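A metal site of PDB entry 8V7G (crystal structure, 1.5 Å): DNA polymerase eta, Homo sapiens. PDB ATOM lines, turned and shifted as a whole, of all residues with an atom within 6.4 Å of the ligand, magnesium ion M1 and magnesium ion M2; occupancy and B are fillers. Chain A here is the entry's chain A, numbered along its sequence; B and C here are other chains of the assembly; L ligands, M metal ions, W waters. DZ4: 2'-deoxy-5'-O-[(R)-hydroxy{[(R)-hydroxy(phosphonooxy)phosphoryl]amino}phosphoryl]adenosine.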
ATOM      1  N   ASP A  16      24.887 -15.746   7.380  1.00  0.00           N
ATOM      2  CA  ASP A  16      25.451 -15.665   8.728  1.00  0.00           C
ATOM      3  C   ASP A  16      24.967 -14.412   9.437  1.00  0.00           C
ATOM      4  O   ASP A  16      25.182 -13.298   8.954  1.00  0.00           O
ATOM      5  CB  ASP A  16      26.985 -15.716   8.691  1.00  0.00           C
ATOM      6  CG  ASP A  16      27.583 -15.896  10.059  1.00  0.00           C
ATOM      7  OD1 ASP A  16      27.481 -14.940  10.840  1.00  0.00           O
ATOM      8  OD2 ASP A  16      28.070 -16.991  10.399  1.00  0.00           O
ATOM      9  N   MET A  17      24.409 -14.607  10.628  1.00  0.00           N
ATOM     10  CA  MET A  17      23.820 -13.475  11.321  1.00  0.00           C
ATOM     11  C   MET A  17      24.943 -12.556  11.793  1.00  0.00           C
ATOM     12  O   MET A  17      26.020 -13.006  12.200  1.00  0.00           O
ATOM     13  CB  MET A  17      22.969 -13.971  12.518  1.00  0.00           C
ATOM     14  CG  MET A  17      21.876 -14.958  12.072  1.00  0.00           C
ATOM     15  SD  MET A  17      20.740 -14.368  10.806  1.00  0.00           S
ATOM     16  CE  MET A  17      19.963 -12.956  11.506  1.00  0.00           C
ATOM     17  N   ASP A  18      24.708 -11.248  11.705  1.00  0.00           N
ATOM     18  CA  ASP A  18      25.679 -10.287  12.222  1.00  0.00           C
ATOM     19  C   ASP A  18      25.620 -10.225  13.740  1.00  0.00           C
ATOM     20  O   ASP A  18      24.531 -10.184  14.317  1.00  0.00           O
ATOM     21  CB  ASP A  18      25.455  -8.893  11.627  1.00  0.00           C
ATOM     22  CG  ASP A  18      25.573  -8.869  10.106  1.00  0.00           C
ATOM     23  OD1 ASP A  18      26.301  -9.696   9.535  1.00  0.00           O
ATOM     24  OD2 ASP A  18      24.936  -8.008   9.485  1.00  0.00           O
ATOM     25  N   CYS A  19      26.792 -10.270  14.388  1.00  0.00           N
ATOM     26  CA  CYS A  19      26.957 -10.203  15.849  1.00  0.00           C
ATOM     27  C   CYS A  19      25.736 -10.780  16.559  1.00  0.00           C
ATOM     28  O   CYS A  19      25.031 -10.070  17.301  1.00  0.00           O
ATOM     29  CB  CYS A  19      27.275  -8.772  16.312  1.00  0.00           C
ATOM     30  SG  CYS A  19      26.214  -7.420  15.813  1.00  0.00           S
ATOM     31  N   PHE A  20      25.465 -12.067  16.343  1.00  0.00           N
ATOM     32  CA  PHE A  20      24.106 -12.604  16.531  1.00  0.00           C
ATOM     33  C   PHE A  20      23.588 -12.438  17.956  1.00  0.00           C
ATOM     34  O   PHE A  20      22.500 -11.883  18.157  1.00  0.00           O
ATOM     35  CB  PHE A  20      24.069 -14.078  16.123  1.00  0.00           C
ATOM     36  CG  PHE A  20      22.712 -14.685  16.238  1.00  0.00           C
ATOM     37  CD1 PHE A  20      21.581 -14.028  15.708  1.00  0.00           C
ATOM     38  CD2 PHE A  20      22.531 -15.916  16.858  1.00  0.00           C
ATOM     39  CE1 PHE A  20      20.304 -14.598  15.812  1.00  0.00           C
ATOM     40  CE2 PHE A  20      21.242 -16.498  16.944  1.00  0.00           C
ATOM     41  CZ  PHE A  20      20.146 -15.837  16.427  1.00  0.00           C
ATOM     42  N   PHE A  21      24.324 -12.922  18.960  1.00  0.00           N
ATOM     43  CA  PHE A  21      23.776 -12.826  20.330  1.00  0.00           C
ATOM     44  C   PHE A  21      23.565 -11.375  20.737  1.00  0.00           C
ATOM     45  O   PHE A  21      22.620 -11.060  21.476  1.00  0.00           O
ATOM     46  CB  PHE A  21      24.681 -13.520  21.352  1.00  0.00           C
ATOM     47  CG  PHE A  21      24.723 -15.020  21.272  1.00  0.00           C
ATOM     48  CD1 PHE A  21      24.261 -15.727  20.167  1.00  0.00           C
ATOM     49  CD2 PHE A  21      25.312 -15.742  22.311  1.00  0.00           C
ATOM     50  CE1 PHE A  21      24.339 -17.143  20.123  1.00  0.00           C
ATOM     51  CE2 PHE A  21      25.396 -17.132  22.257  1.00  0.00           C
ATOM     52  CZ  PHE A  21      24.908 -17.833  21.170  1.00  0.00           C
ATOM     53  N   VAL A  22      24.436 -10.465  20.288  1.00  0.00           N
ATOM     54  CA  VAL A  22      24.215  -9.049  20.546  1.00  0.00           C
ATOM     55  C   VAL A  22      22.893  -8.579  19.921  1.00  0.00           C
ATOM     56  O   VAL A  22      22.103  -7.886  20.568  1.00  0.00           O
ATOM     57  CB  VAL A  22      25.395  -8.219  20.023  1.00  0.00           C
ATOM     58  CG1 VAL A  22      25.022  -6.726  19.991  1.00  0.00           C
ATOM     59  CG2 VAL A  22      26.648  -8.460  20.871  1.00  0.00           C
ATOM     60  N   GLN A  41      29.365 -14.040  29.439  1.00  0.00           N
ATOM     61  CA  GLN A  41      28.999 -15.215  30.229  1.00  0.00           C
ATOM     62  C   GLN A  41      29.683 -15.127  31.576  1.00  0.00           C
ATOM     63  O   GLN A  41      30.907 -14.972  31.634  1.00  0.00           O
ATOM     64  CB  GLN A  41      29.406 -16.530  29.552  1.00  0.00           C
ATOM     65  CG  GLN A  41      28.454 -17.028  28.512  1.00  0.00           C
ATOM     66  CD  GLN A  41      28.852 -18.377  27.937  1.00  0.00           C
ATOM     67  OE1 GLN A  41      27.981 -19.186  27.605  1.00  0.00           O
ATOM     68  NE2 GLN A  41      30.149 -18.629  27.819  1.00  0.00           N
ATOM     69  N   ILE A  51      31.426 -13.251  24.500  1.00  0.00           N
ATOM     70  CA  ILE A  51      31.190 -14.201  23.427  1.00  0.00           C
ATOM     71  C   ILE A  51      30.620 -13.580  22.156  1.00  0.00           C
ATOM     72  O   ILE A  51      30.606 -14.257  21.120  1.00  0.00           O
ATOM     73  CB  ILE A  51      30.311 -15.383  23.880  1.00  0.00           C
ATOM     74  CG1 ILE A  51      28.945 -14.923  24.400  1.00  0.00           C
ATOM     75  CG2 ILE A  51      31.076 -16.229  24.920  1.00  0.00           C
ATOM     76  CD1 ILE A  51      27.992 -16.098  24.633  1.00  0.00           C
ATOM     77  N   ALA A  52      30.195 -12.312  22.176  1.00  0.00           N
ATOM     78  CA  ALA A  52      29.699 -11.626  20.975  1.00  0.00           C
ATOM     79  C   ALA A  52      29.873 -10.130  21.162  1.00  0.00           C
ATOM     80  O   ALA A  52      29.768  -9.631  22.281  1.00  0.00           O
ATOM     81  CB  ALA A  52      28.224 -11.954  20.684  1.00  0.00           C
ATOM     82  N   VAL A  53      30.156  -9.410  20.055  1.00  0.00           N
ATOM     83  CA  VAL A  53      30.582  -8.013  20.085  1.00  0.00           C
ATOM     84  C   VAL A  53      29.915  -7.244  18.959  1.00  0.00           C
ATOM     85  O   VAL A  53      30.025  -7.631  17.788  1.00  0.00           O
ATOM     86  CB  VAL A  53      32.109  -7.910  19.942  1.00  0.00           C
ATOM     87  CG1 VAL A  53      32.543  -6.479  20.135  1.00  0.00           C
ATOM     88  CG2 VAL A  53      32.811  -8.769  20.949  1.00  0.00           C
ATOM     89  N   TYR A  55      29.398  -4.219  16.226  1.00  0.00           N
ATOM     90  CA  TYR A  55      30.411  -3.643  15.345  1.00  0.00           C
ATOM     91  C   TYR A  55      30.927  -2.304  15.880  1.00  0.00           C
ATOM     92  O   TYR A  55      32.126  -1.995  15.743  1.00  0.00           O
ATOM     93  CB  TYR A  55      29.859  -3.551  13.910  1.00  0.00           C
ATOM     94  CG  TYR A  55      29.916  -4.908  13.214  1.00  0.00           C
ATOM     95  CD1 TYR A  55      28.950  -5.899  13.466  1.00  0.00           C
ATOM     96  CD2 TYR A  55      30.993  -5.247  12.386  1.00  0.00           C
ATOM     97  CE1 TYR A  55      29.034  -7.167  12.870  1.00  0.00           C
ATOM     98  CE2 TYR A  55      31.087  -6.496  11.788  1.00  0.00           C
ATOM     99  CZ  TYR A  55      30.116  -7.452  12.042  1.00  0.00           C
ATOM    100  OH  TYR A  55      30.247  -8.695  11.443  1.00  0.00           O
ATOM    101  N   ARG A  58      33.535  -3.354  18.229  1.00  0.00           N
ATOM    102  CA  ARG A  58      34.717  -3.862  17.515  1.00  0.00           C
ATOM    103  C   ARG A  58      35.634  -2.722  17.063  1.00  0.00           C
ATOM    104  O   ARG A  58      36.857  -2.905  17.026  1.00  0.00           O
ATOM    105  CB  ARG A  58      34.299  -4.707  16.316  1.00  0.00           C
ATOM    106  CG  ARG A  58      33.577  -6.009  16.673  1.00  0.00           C
ATOM    107  CD  ARG A  58      33.175  -6.753  15.423  1.00  0.00           C
ATOM    108  NE  ARG A  58      32.103  -7.705  15.719  1.00  0.00           N
ATOM    109  CZ  ARG A  58      31.791  -8.761  14.989  1.00  0.00           C
ATOM    110  NH1 ARG A  58      32.431  -9.033  13.859  1.00  0.00           N
ATOM    111  NH2 ARG A  58      30.778  -9.547  15.363  1.00  0.00           N
ATOM    112  N   ARG A  64      35.699 -11.198  20.906  1.00  0.00           N
ATOM    113  CA  ARG A  64      35.292 -12.405  21.650  1.00  0.00           C
ATOM    114  C   ARG A  64      36.505 -12.984  22.382  1.00  0.00           C
ATOM    115  O   ARG A  64      37.624 -12.748  21.906  1.00  0.00           O
ATOM    116  CB  ARG A  64      34.721 -13.426  20.651  1.00  0.00           C
ATOM    117  CG  ARG A  64      34.448 -14.808  21.210  1.00  0.00           C
ATOM    118  CD  ARG A  64      34.026 -15.704  20.054  1.00  0.00           C
ATOM    119  NE  ARG A  64      35.090 -15.857  19.079  1.00  0.00           N
ATOM    120  CZ  ARG A  64      34.971 -15.619  17.775  1.00  0.00           C
ATOM    121  NH1 ARG A  64      33.817 -15.238  17.268  1.00  0.00           N
ATOM    122  NH2 ARG A  64      36.015 -15.772  16.977  1.00  0.00           N
ATOM    123  N   LEU A  92      21.769 -21.212  27.102  1.00  0.00           N
ATOM    124  CA  LEU A  92      21.759 -20.557  25.789  1.00  0.00           C
ATOM    125  C   LEU A  92      20.377 -20.608  25.104  1.00  0.00           C
ATOM    126  O   LEU A  92      20.288 -20.327  23.902  1.00  0.00           O
ATOM    127  CB  LEU A  92      22.835 -21.184  24.893  1.00  0.00           C
ATOM    128  CG  LEU A  92      24.261 -21.194  25.478  1.00  0.00           C
ATOM    129  CD1 LEU A  92      25.229 -21.954  24.571  1.00  0.00           C
ATOM    130  CD2 LEU A  92      24.731 -19.757  25.671  1.00  0.00           C
ATOM    131  N   SER A 116      25.651 -23.636  11.993  1.00  0.00           N
ATOM    132  CA  SER A 116      25.913 -23.255  13.382  1.00  0.00           C
ATOM    133  C   SER A 116      24.647 -22.610  13.917  1.00  0.00           C
ATOM    134  O   SER A 116      23.677 -22.416  13.190  1.00  0.00           O
ATOM    135  CB  SER A 116      27.103 -22.296  13.517  1.00  0.00           C
ATOM    136  OG  SER A 116      26.722 -20.963  13.192  1.00  0.00           O
ATOM    137  N   ILE A 117      24.713 -22.167  15.181  1.00  0.00           N
ATOM    138  CA  ILE A 117      23.563 -21.497  15.774  1.00  0.00           C
ATOM    139  C   ILE A 117      23.128 -20.276  14.952  1.00  0.00           C
ATOM    140  O   ILE A 117      21.959 -19.885  14.991  1.00  0.00           O
ATOM    141  CB  ILE A 117      23.861 -21.116  17.241  1.00  0.00           C
ATOM    142  CG1 ILE A 117      22.562 -20.799  17.972  1.00  0.00           C
ATOM    143  CG2 ILE A 117      24.826 -19.936  17.313  1.00  0.00           C
ATOM    144  CD1 ILE A 117      22.695 -20.819  19.491  1.00  0.00           C
ATOM    145  N   ASP A 118      24.047 -19.638  14.199  1.00  0.00           N
ATOM    146  CA  ASP A 118      23.654 -18.441  13.461  1.00  0.00           C
ATOM    147  C   ASP A 118      23.915 -18.525  11.959  1.00  0.00           C
ATOM    148  O   ASP A 118      23.888 -17.474  11.285  1.00  0.00           O
ATOM    149  CB  ASP A 118      24.309 -17.191  14.059  1.00  0.00           C
ATOM    150  CG  ASP A 118      25.654 -16.853  13.437  1.00  0.00           C
ATOM    151  OD1 ASP A 118      26.436 -17.774  13.109  1.00  0.00           O
ATOM    152  OD2 ASP A 118      25.937 -15.631  13.258  1.00  0.00           O
ATOM    153  N   GLU A 119      24.107 -19.707  11.391  1.00  0.00           N
ATOM    154  CA  GLU A 119      24.348 -19.699   9.946  1.00  0.00           C
ATOM    155  C   GLU A 119      23.850 -20.968   9.306  1.00  0.00           C
ATOM    156  O   GLU A 119      23.848 -22.047   9.929  1.00  0.00           O
ATOM    157  CB  GLU A 119      25.816 -19.566   9.552  1.00  0.00           C
ATOM    158  CG  GLU A 119      26.678 -20.602  10.176  1.00  0.00           C
ATOM    159  CD  GLU A 119      28.122 -20.197  10.254  1.00  0.00           C
ATOM    160  OE1 GLU A 119      28.864 -20.169   9.247  1.00  0.00           O
ATOM    161  OE2 GLU A 119      28.453 -19.733  11.354  1.00  0.00           O
ATOM    162  N   SER A 216      24.613 -11.140   7.002  1.00  0.00           N
ATOM    163  CA  SER A 216      25.385 -11.065   5.767  1.00  0.00           C
ATOM    164  C   SER A 216      25.294 -12.398   5.057  1.00  0.00           C
ATOM    165  O   SER A 216      24.855 -13.390   5.618  1.00  0.00           O
ATOM    166  CB  SER A 216      26.838 -10.681   6.047  1.00  0.00           C
ATOM    167  OG  SER A 216      26.878  -9.437   6.739  1.00  0.00           O
ATOM    168  N   LYS A 227      30.920 -19.390   2.058  1.00  0.00           N
ATOM    169  CA  LYS A 227      31.322 -18.994   3.400  1.00  0.00           C
ATOM    170  C   LYS A 227      32.403 -17.914   3.343  1.00  0.00           C
ATOM    171  O   LYS A 227      32.321 -16.902   4.061  1.00  0.00           O
ATOM    172  CB  LYS A 227      31.808 -20.216   4.194  1.00  0.00           C
ATOM    173  CG  LYS A 227      32.436 -19.878   5.538  1.00  0.00           C
ATOM    174  CD  LYS A 227      31.403 -19.314   6.498  1.00  0.00           C
ATOM    175  CE  LYS A 227      32.013 -19.081   7.863  1.00  0.00           C
ATOM    176  NZ  LYS A 227      31.028 -18.510   8.833  1.00  0.00           N
ATOM    177  N   LYS A 234      30.891  -8.100   5.567  1.00  0.00           N
ATOM    178  CA  LYS A 234      30.123  -7.927   6.794  1.00  0.00           C
ATOM    179  C   LYS A 234      30.338  -6.521   7.360  1.00  0.00           C
ATOM    180  O   LYS A 234      31.450  -5.980   7.291  1.00  0.00           O
ATOM    181  CB  LYS A 234      30.594  -8.948   7.818  1.00  0.00           C
ATOM    182  CG  LYS A 234      29.937 -10.295   7.727  1.00  0.00           C
ATOM    183  CD  LYS A 234      30.093 -11.105   9.003  1.00  0.00           C
ATOM    184  CE  LYS A 234      29.079 -12.290   9.024  1.00  0.00           C
ATOM    185  NZ  LYS A 234      27.816 -12.023   9.806  1.00  0.00           N
ATOM    186  N   PRO A 235      29.328  -5.921   8.004  1.00  0.00           N
ATOM    187  CA  PRO A 235      27.980  -6.474   8.256  1.00  0.00           C
ATOM    188  C   PRO A 235      26.934  -5.982   7.268  1.00  0.00           C
ATOM    189  O   PRO A 235      27.124  -5.003   6.521  1.00  0.00           O
ATOM    190  CB  PRO A 235      27.658  -5.946   9.653  1.00  0.00           C
ATOM    191  CG  PRO A 235      28.296  -4.572   9.664  1.00  0.00           C
ATOM    192  CD  PRO A 235      29.557  -4.716   8.817  1.00  0.00           C
ATOM    193  P   U7B B   8      33.957 -19.936  11.920  1.00  0.00           P
ATOM    194  C5' U7B B   8      31.415 -20.670  12.411  1.00  0.00           C
ATOM    195  O5' U7B B   8      32.592 -19.986  12.845  1.00  0.00           O
ATOM    196  C4' U7B B   8      30.634 -21.012  13.587  1.00  0.00           C
ATOM    197  O4' U7B B   8      31.486 -21.701  14.529  1.00  0.00           O
ATOM    198  C3' U7B B   8      30.230 -19.758  14.366  1.00  0.00           C
ATOM    199  O3' U7B B   8      28.968 -19.225  13.873  1.00  0.00           O
ATOM    200  C2' U7B B   8      30.029 -20.305  15.808  1.00  0.00           C
ATOM    201  C1' U7B B   8      30.879 -21.666  15.810  1.00  0.00           C
ATOM    202  N1  U7B B   8      31.923 -21.759  16.792  1.00  0.00           N
ATOM    203  C2  U7B B   8      31.602 -22.125  18.082  1.00  0.00           C
ATOM    204  O2  U7B B   8      30.433 -22.308  18.391  1.00  0.00           O
ATOM    205  N3  U7B B   8      32.582 -22.281  19.003  1.00  0.00           N
ATOM    206  C4  U7B B   8      33.850 -22.082  18.685  1.00  0.00           C
ATOM    207  N4  U7B B   8      34.784 -22.234  19.606  1.00  0.00           N
ATOM    208  C5  U7B B   8      34.199 -21.709  17.370  1.00  0.00           C
ATOM    209  C6  U7B B   8      33.235 -21.567  16.443  1.00  0.00           C
ATOM    210  OP1 U7B B   8      33.639 -19.271  10.609  1.00  0.00           O
ATOM    211  OP2 U7B B   8      35.043 -19.235  12.680  1.00  0.00           O
ATOM    212  F1  U7B B   8      28.724 -20.624  16.006  1.00  0.00           F
ATOM    213  F2  U7B B   8      30.400 -19.428  16.751  1.00  0.00           F
ATOM    214  P    DT C   4      37.141 -21.340  31.073  1.00  0.00           P
ATOM    215  OP1  DT C   4      36.818 -21.173  32.510  1.00  0.00           O
ATOM    216  OP2  DT C   4      37.833 -22.569  30.610  1.00  0.00           O
ATOM    217  O5'  DT C   4      35.791 -21.181  30.251  1.00  0.00           O
ATOM    218  C5'  DT C   4      34.887 -20.142  30.557  1.00  0.00           C
ATOM    219  C4'  DT C   4      33.528 -20.450  29.970  1.00  0.00           C
ATOM    220  O4'  DT C   4      33.524 -20.156  28.568  1.00  0.00           O
ATOM    221  C3'  DT C   4      33.076 -21.905  30.088  1.00  0.00           C
ATOM    222  O3'  DT C   4      31.730 -21.885  30.433  1.00  0.00           O
ATOM    223  C2'  DT C   4      33.319 -22.480  28.680  1.00  0.00           C
ATOM    224  C1'  DT C   4      33.026 -21.252  27.832  1.00  0.00           C
ATOM    225  N1   DT C   4      33.687 -21.218  26.523  1.00  0.00           N
ATOM    226  C2   DT C   4      32.983 -20.685  25.487  1.00  0.00           C
ATOM    227  O2   DT C   4      31.826 -20.298  25.601  1.00  0.00           O
ATOM    228  N3   DT C   4      33.648 -20.631  24.305  1.00  0.00           N
ATOM    229  C4   DT C   4      34.944 -21.019  24.048  1.00  0.00           C
ATOM    230  O4   DT C   4      35.449 -20.908  22.939  1.00  0.00           O
ATOM    231  C5   DT C   4      35.663 -21.552  25.187  1.00  0.00           C
ATOM    232  C7   DT C   4      37.078 -22.017  25.028  1.00  0.00           C
ATOM    233  C6   DT C   4      35.001 -21.623  26.368  1.00  0.00           C
ATOM    234  P    DG C   5      30.910 -23.234  30.690  1.00  0.00           P
ATOM    235  OP1  DG C   5      30.006 -22.999  31.830  1.00  0.00           O
ATOM    236  OP2  DG C   5      31.863 -24.358  30.721  1.00  0.00           O
ATOM    237  O5'  DG C   5      30.048 -23.375  29.352  1.00  0.00           O
ATOM    238  C5'  DG C   5      29.022 -22.441  29.065  1.00  0.00           C
ATOM    239  C4'  DG C   5      28.357 -22.812  27.769  1.00  0.00           C
ATOM    240  O4'  DG C   5      29.295 -22.611  26.676  1.00  0.00           O
ATOM    241  C3'  DG C   5      27.920 -24.282  27.672  1.00  0.00           C
ATOM    242  O3'  DG C   5      26.702 -24.344  26.947  1.00  0.00           O
ATOM    243  C2'  DG C   5      29.062 -24.919  26.886  1.00  0.00           C
ATOM    244  C1'  DG C   5      29.347 -23.799  25.911  1.00  0.00           C
ATOM    245  N9   DG C   5      30.624 -23.881  25.260  1.00  0.00           N
ATOM    246  C8   DG C   5      31.808 -24.369  25.774  1.00  0.00           C
ATOM    247  N7   DG C   5      32.808 -24.314  24.920  1.00  0.00           N
ATOM    248  C5   DG C   5      32.230 -23.763  23.776  1.00  0.00           C
ATOM    249  C6   DG C   5      32.801 -23.470  22.504  1.00  0.00           C
ATOM    250  O6   DG C   5      33.969 -23.633  22.122  1.00  0.00           O
ATOM    251  N1   DG C   5      31.863 -22.918  21.634  1.00  0.00           N
ATOM    252  C2   DG C   5      30.557 -22.695  21.943  1.00  0.00           C
ATOM    253  N2   DG C   5      29.802 -22.159  20.978  1.00  0.00           N
ATOM    254  N3   DG C   5      30.005 -22.964  23.113  1.00  0.00           N
ATOM    255  C4   DG C   5      30.912 -23.497  23.973  1.00  0.00           C
HETATM  256  N1  DZ4 L   1      32.098 -19.551  22.290  1.00  0.00           N
HETATM  257  C2  DZ4 L   1      30.806 -19.384  22.588  1.00  0.00           C
HETATM  258  N3  DZ4 L   1      29.924 -18.784  21.811  1.00  0.00           N
HETATM  259  C4  DZ4 L   1      30.390 -18.333  20.626  1.00  0.00           C
HETATM  260  C5  DZ4 L   1      31.730 -18.469  20.246  1.00  0.00           C
HETATM  261  C6  DZ4 L   1      32.595 -19.109  21.123  1.00  0.00           C
HETATM  262  N6  DZ4 L   1      33.898 -19.276  20.834  1.00  0.00           N
HETATM  263  N7  DZ4 L   1      31.861 -17.909  19.017  1.00  0.00           N
HETATM  264  C8  DZ4 L   1      30.648 -17.432  18.649  1.00  0.00           C
HETATM  265  N9  DZ4 L   1      29.763 -17.686  19.629  1.00  0.00           N
HETATM  266  PA  DZ4 L   1      29.698 -15.941  14.774  1.00  0.00           P
HETATM  267  PB  DZ4 L   1      28.783 -13.205  15.389  1.00  0.00           P
HETATM  268  PG  DZ4 L   1      29.693 -11.908  12.936  1.00  0.00           P
HETATM  269  C1' DZ4 L   1      28.319 -17.344  19.604  1.00  0.00           C
HETATM  270  O1A DZ4 L   1      28.888 -15.978  13.550  1.00  0.00           O
HETATM  271  O1B DZ4 L   1      27.533 -13.637  14.741  1.00  0.00           O
HETATM  272  O1G DZ4 L   1      29.101 -13.147  12.327  1.00  0.00           O
HETATM  273  C2' DZ4 L   1      28.025 -15.856  19.765  1.00  0.00           C
HETATM  274  O2A DZ4 L   1      31.134 -16.581  14.642  1.00  0.00           O
HETATM  275  O2B DZ4 L   1      28.668 -12.664  16.814  1.00  0.00           O
HETATM  276  O2G DZ4 L   1      28.966 -10.636  12.489  1.00  0.00           O
HETATM  277  C3' DZ4 L   1      27.902 -15.384  18.319  1.00  0.00           C
HETATM  278  O3' DZ4 L   1      27.027 -14.256  18.251  1.00  0.00           O
HETATM  279  N3A DZ4 L   1      29.915 -14.397  15.312  1.00  0.00           N
HETATM  280  O3B DZ4 L   1      29.427 -12.011  14.553  1.00  0.00           O
HETATM  281  O3G DZ4 L   1      31.229 -11.738  12.787  1.00  0.00           O
HETATM  282  C4' DZ4 L   1      27.241 -16.602  17.680  1.00  0.00           C
HETATM  283  O4' DZ4 L   1      27.786 -17.763  18.354  1.00  0.00           O
HETATM  284  C5' DZ4 L   1      27.566 -16.703  16.158  1.00  0.00           C
HETATM  285  O5' DZ4 L   1      28.973 -16.766  15.955  1.00  0.00           O
HETATM  286 MG    MG M   1      28.455 -17.808  12.318  1.00  0.00          MG
HETATM  287 MG    MG M   2      27.491 -14.422  12.780  1.00  0.00          MG
HETATM  288  O   HOH W   1      31.461 -14.206  18.036  1.00  0.00           O
HETATM  289  O   HOH W   2      30.566 -11.030  17.788  1.00  0.00           O
HETATM  290  O   HOH W   3      33.039 -12.544  14.485  1.00  0.00           O
HETATM  291  O   HOH W   4      28.084 -20.610  18.585  1.00  0.00           O
HETATM  292  O   HOH W   5      30.809 -14.886  10.928  1.00  0.00           O
HETATM  293  O   HOH W   6      32.989 -18.017  16.386  1.00  0.00           O
HETATM  294  O   HOH W   7      30.548 -17.553  11.794  1.00  0.00           O
HETATM  295  O   HOH W   8      33.102 -10.918  11.000  1.00  0.00           O
HETATM  296  O   HOH W   9      27.515 -19.717  22.893  1.00  0.00           O
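A nitrogen (N1) of the ligand lies close to N1 of DG 5 of chain C. Asp 18 touches the ligand. Ile 51 touches the ligand (O to C2', 3.3 Å). Ala 52 touches the ligand. Ile 117 touches the ligand (CG2 to O4', 3.8 Å). Within 4 Å of the ligand: Asp 16, Met 17, Asp 18, Cys 19, Phe 20, Phe 21, Ile 51, Ala 52, Tyr 55, Arg 58, Arg 64, Ile 117, Asp 118, Lys 234, U7B 8 of chain B, DT 4 of chain C and DG 5 of chain C. The nearest printed residue that does not touch the ligand is Glu 119 (4.4 Å).
O3' of U7B 8 of chain B lies close to the side-chain hydroxyl of Ser 116, at 2.9 Å. The backbone carbonyl oxygen of Met 17 lies close to the side-chain amino group of Lys 234. N of Asp 16 is in hydrogen-bond range of O of Ser 216, 2.9 Å away. NE of Arg 58 is in hydrogen-bond range of O of Val 53 (2.9 Å). OH of Tyr 55 sits at hydrogen-bond distance from NH1 of Arg 58 (3.3 Å). The side-chain amide nitrogen (NE2) of Gln 41 lies within hydrogen-bond range of O2 of DT 4 of chain C, at 3.2 Å. OD1 of Asp 18 sits at hydrogen-bond distance from OG of Ser 216. O of Asp 16 sits at hydrogen-bond distance from NZ of Lys 234.
Ser 116 touches magnesium ion M1. Along chain A the residues within 4 Å of magnesium ion M1 span positions 16 to 119. The nearest printed residue that does not touch magnesium ion M1 is Lys 227 (4.4 Å).
Water W7 lies within hydrogen-bond range of an oxygen (O2A) of the ligand (3.1 Å), the side-chain amino group (NZ) of Lys 227 (3.1 Å) and O5' of U7B 8 of chain B (3.3 Å). Water W2 lies within hydrogen-bond range of an oxygen (O2B) of the ligand (2.7 Å), the backbone NH of Val 53 (2.8 Å) and the guanidinium group of Arg 58 (2.9 Å). Water W8 lies within hydrogen-bond range of O3G of the ligand (2.7 Å) and NH1 of Arg 58 (3.5 Å). Water W6 bridges N7 of the ligand and NH1 of Arg 64. Water W1 lies within hydrogen-bond range of NH1 of Arg 64 (2.7 Å), N3A of the ligand (3.1 Å) and O of Ile 51 (3.2 Å).
Magnesium ion M2 is bound by the side-chain carboxylate (OD1) of Asp 16, the side-chain carboxylate (OD2) of Asp 118, an oxygen (O1G) of the ligand, an oxygen (O1B) of the ligand, the backbone carbonyl oxygen (O) of Met 17 and an oxygen (O1A) of the ligand.
OH of Tyr 55 sits at hydrogen-bond distance from O2G of the ligand (2.6 Å). The guanidinium group (NH1) of Arg 58 lies within salt-bridge range of an oxygen (O3G) of the ligand. A nitrogen (N6) of the ligand is in hydrogen-bond range of N4 of U7B 8 of chain B (3.3 Å). The side-chain amino group (NZ) of Lys 234 lies within salt-bridge range of an oxygen (O2G) of the ligand (3.2 Å). The backbone NH (N) of Phe 21 lies within hydrogen-bond range of an oxygen (O3') of the ligand, at 3.1 Å. NH1 of Arg 64 is in salt-bridge range of O2A of the ligand (3.99 Å). The backbone NH (N) of Phe 20 lies within hydrogen-bond range of an oxygen (O2B) of the ligand. O2G of the ligand is in hydrogen-bond range of N of Cys 19 (2.9 Å). N6 of the ligand lies within hydrogen-bond range of O4 of DT 4 of chain C (3.1 Å).
The side-chain carboxylate (OD2) of Asp 16 is bound to magnesium ion M1. Magnesium ion M1 is bound by OE2 of Glu 119, at 2.2 Å. O3' of U7B 8 of chain B binds magnesium ion M1, at 2.2 Å. OD1 of Asp 118 is bound to magnesium ion M1, at 2.2 Å. Magnesium ion M1 is bound by water W7, 2.2 Å away. O1A of the ligand is bound to magnesium ion M1, 2.2 Å away. Magnesium ion M1 has six donor atoms within binding distance.
Residues that only touch magnesium ion M2: Lys 234. Within 4 Å of magnesium ion M2: Asp 16, Met 17, Asp 118 and Lys 234. Along chain A the residues within 4 Å of magnesium ion M2 span positions 16 to 234. The nearest printed residue that does not touch magnesium ion M2 is Asp 18 (4.4 Å).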
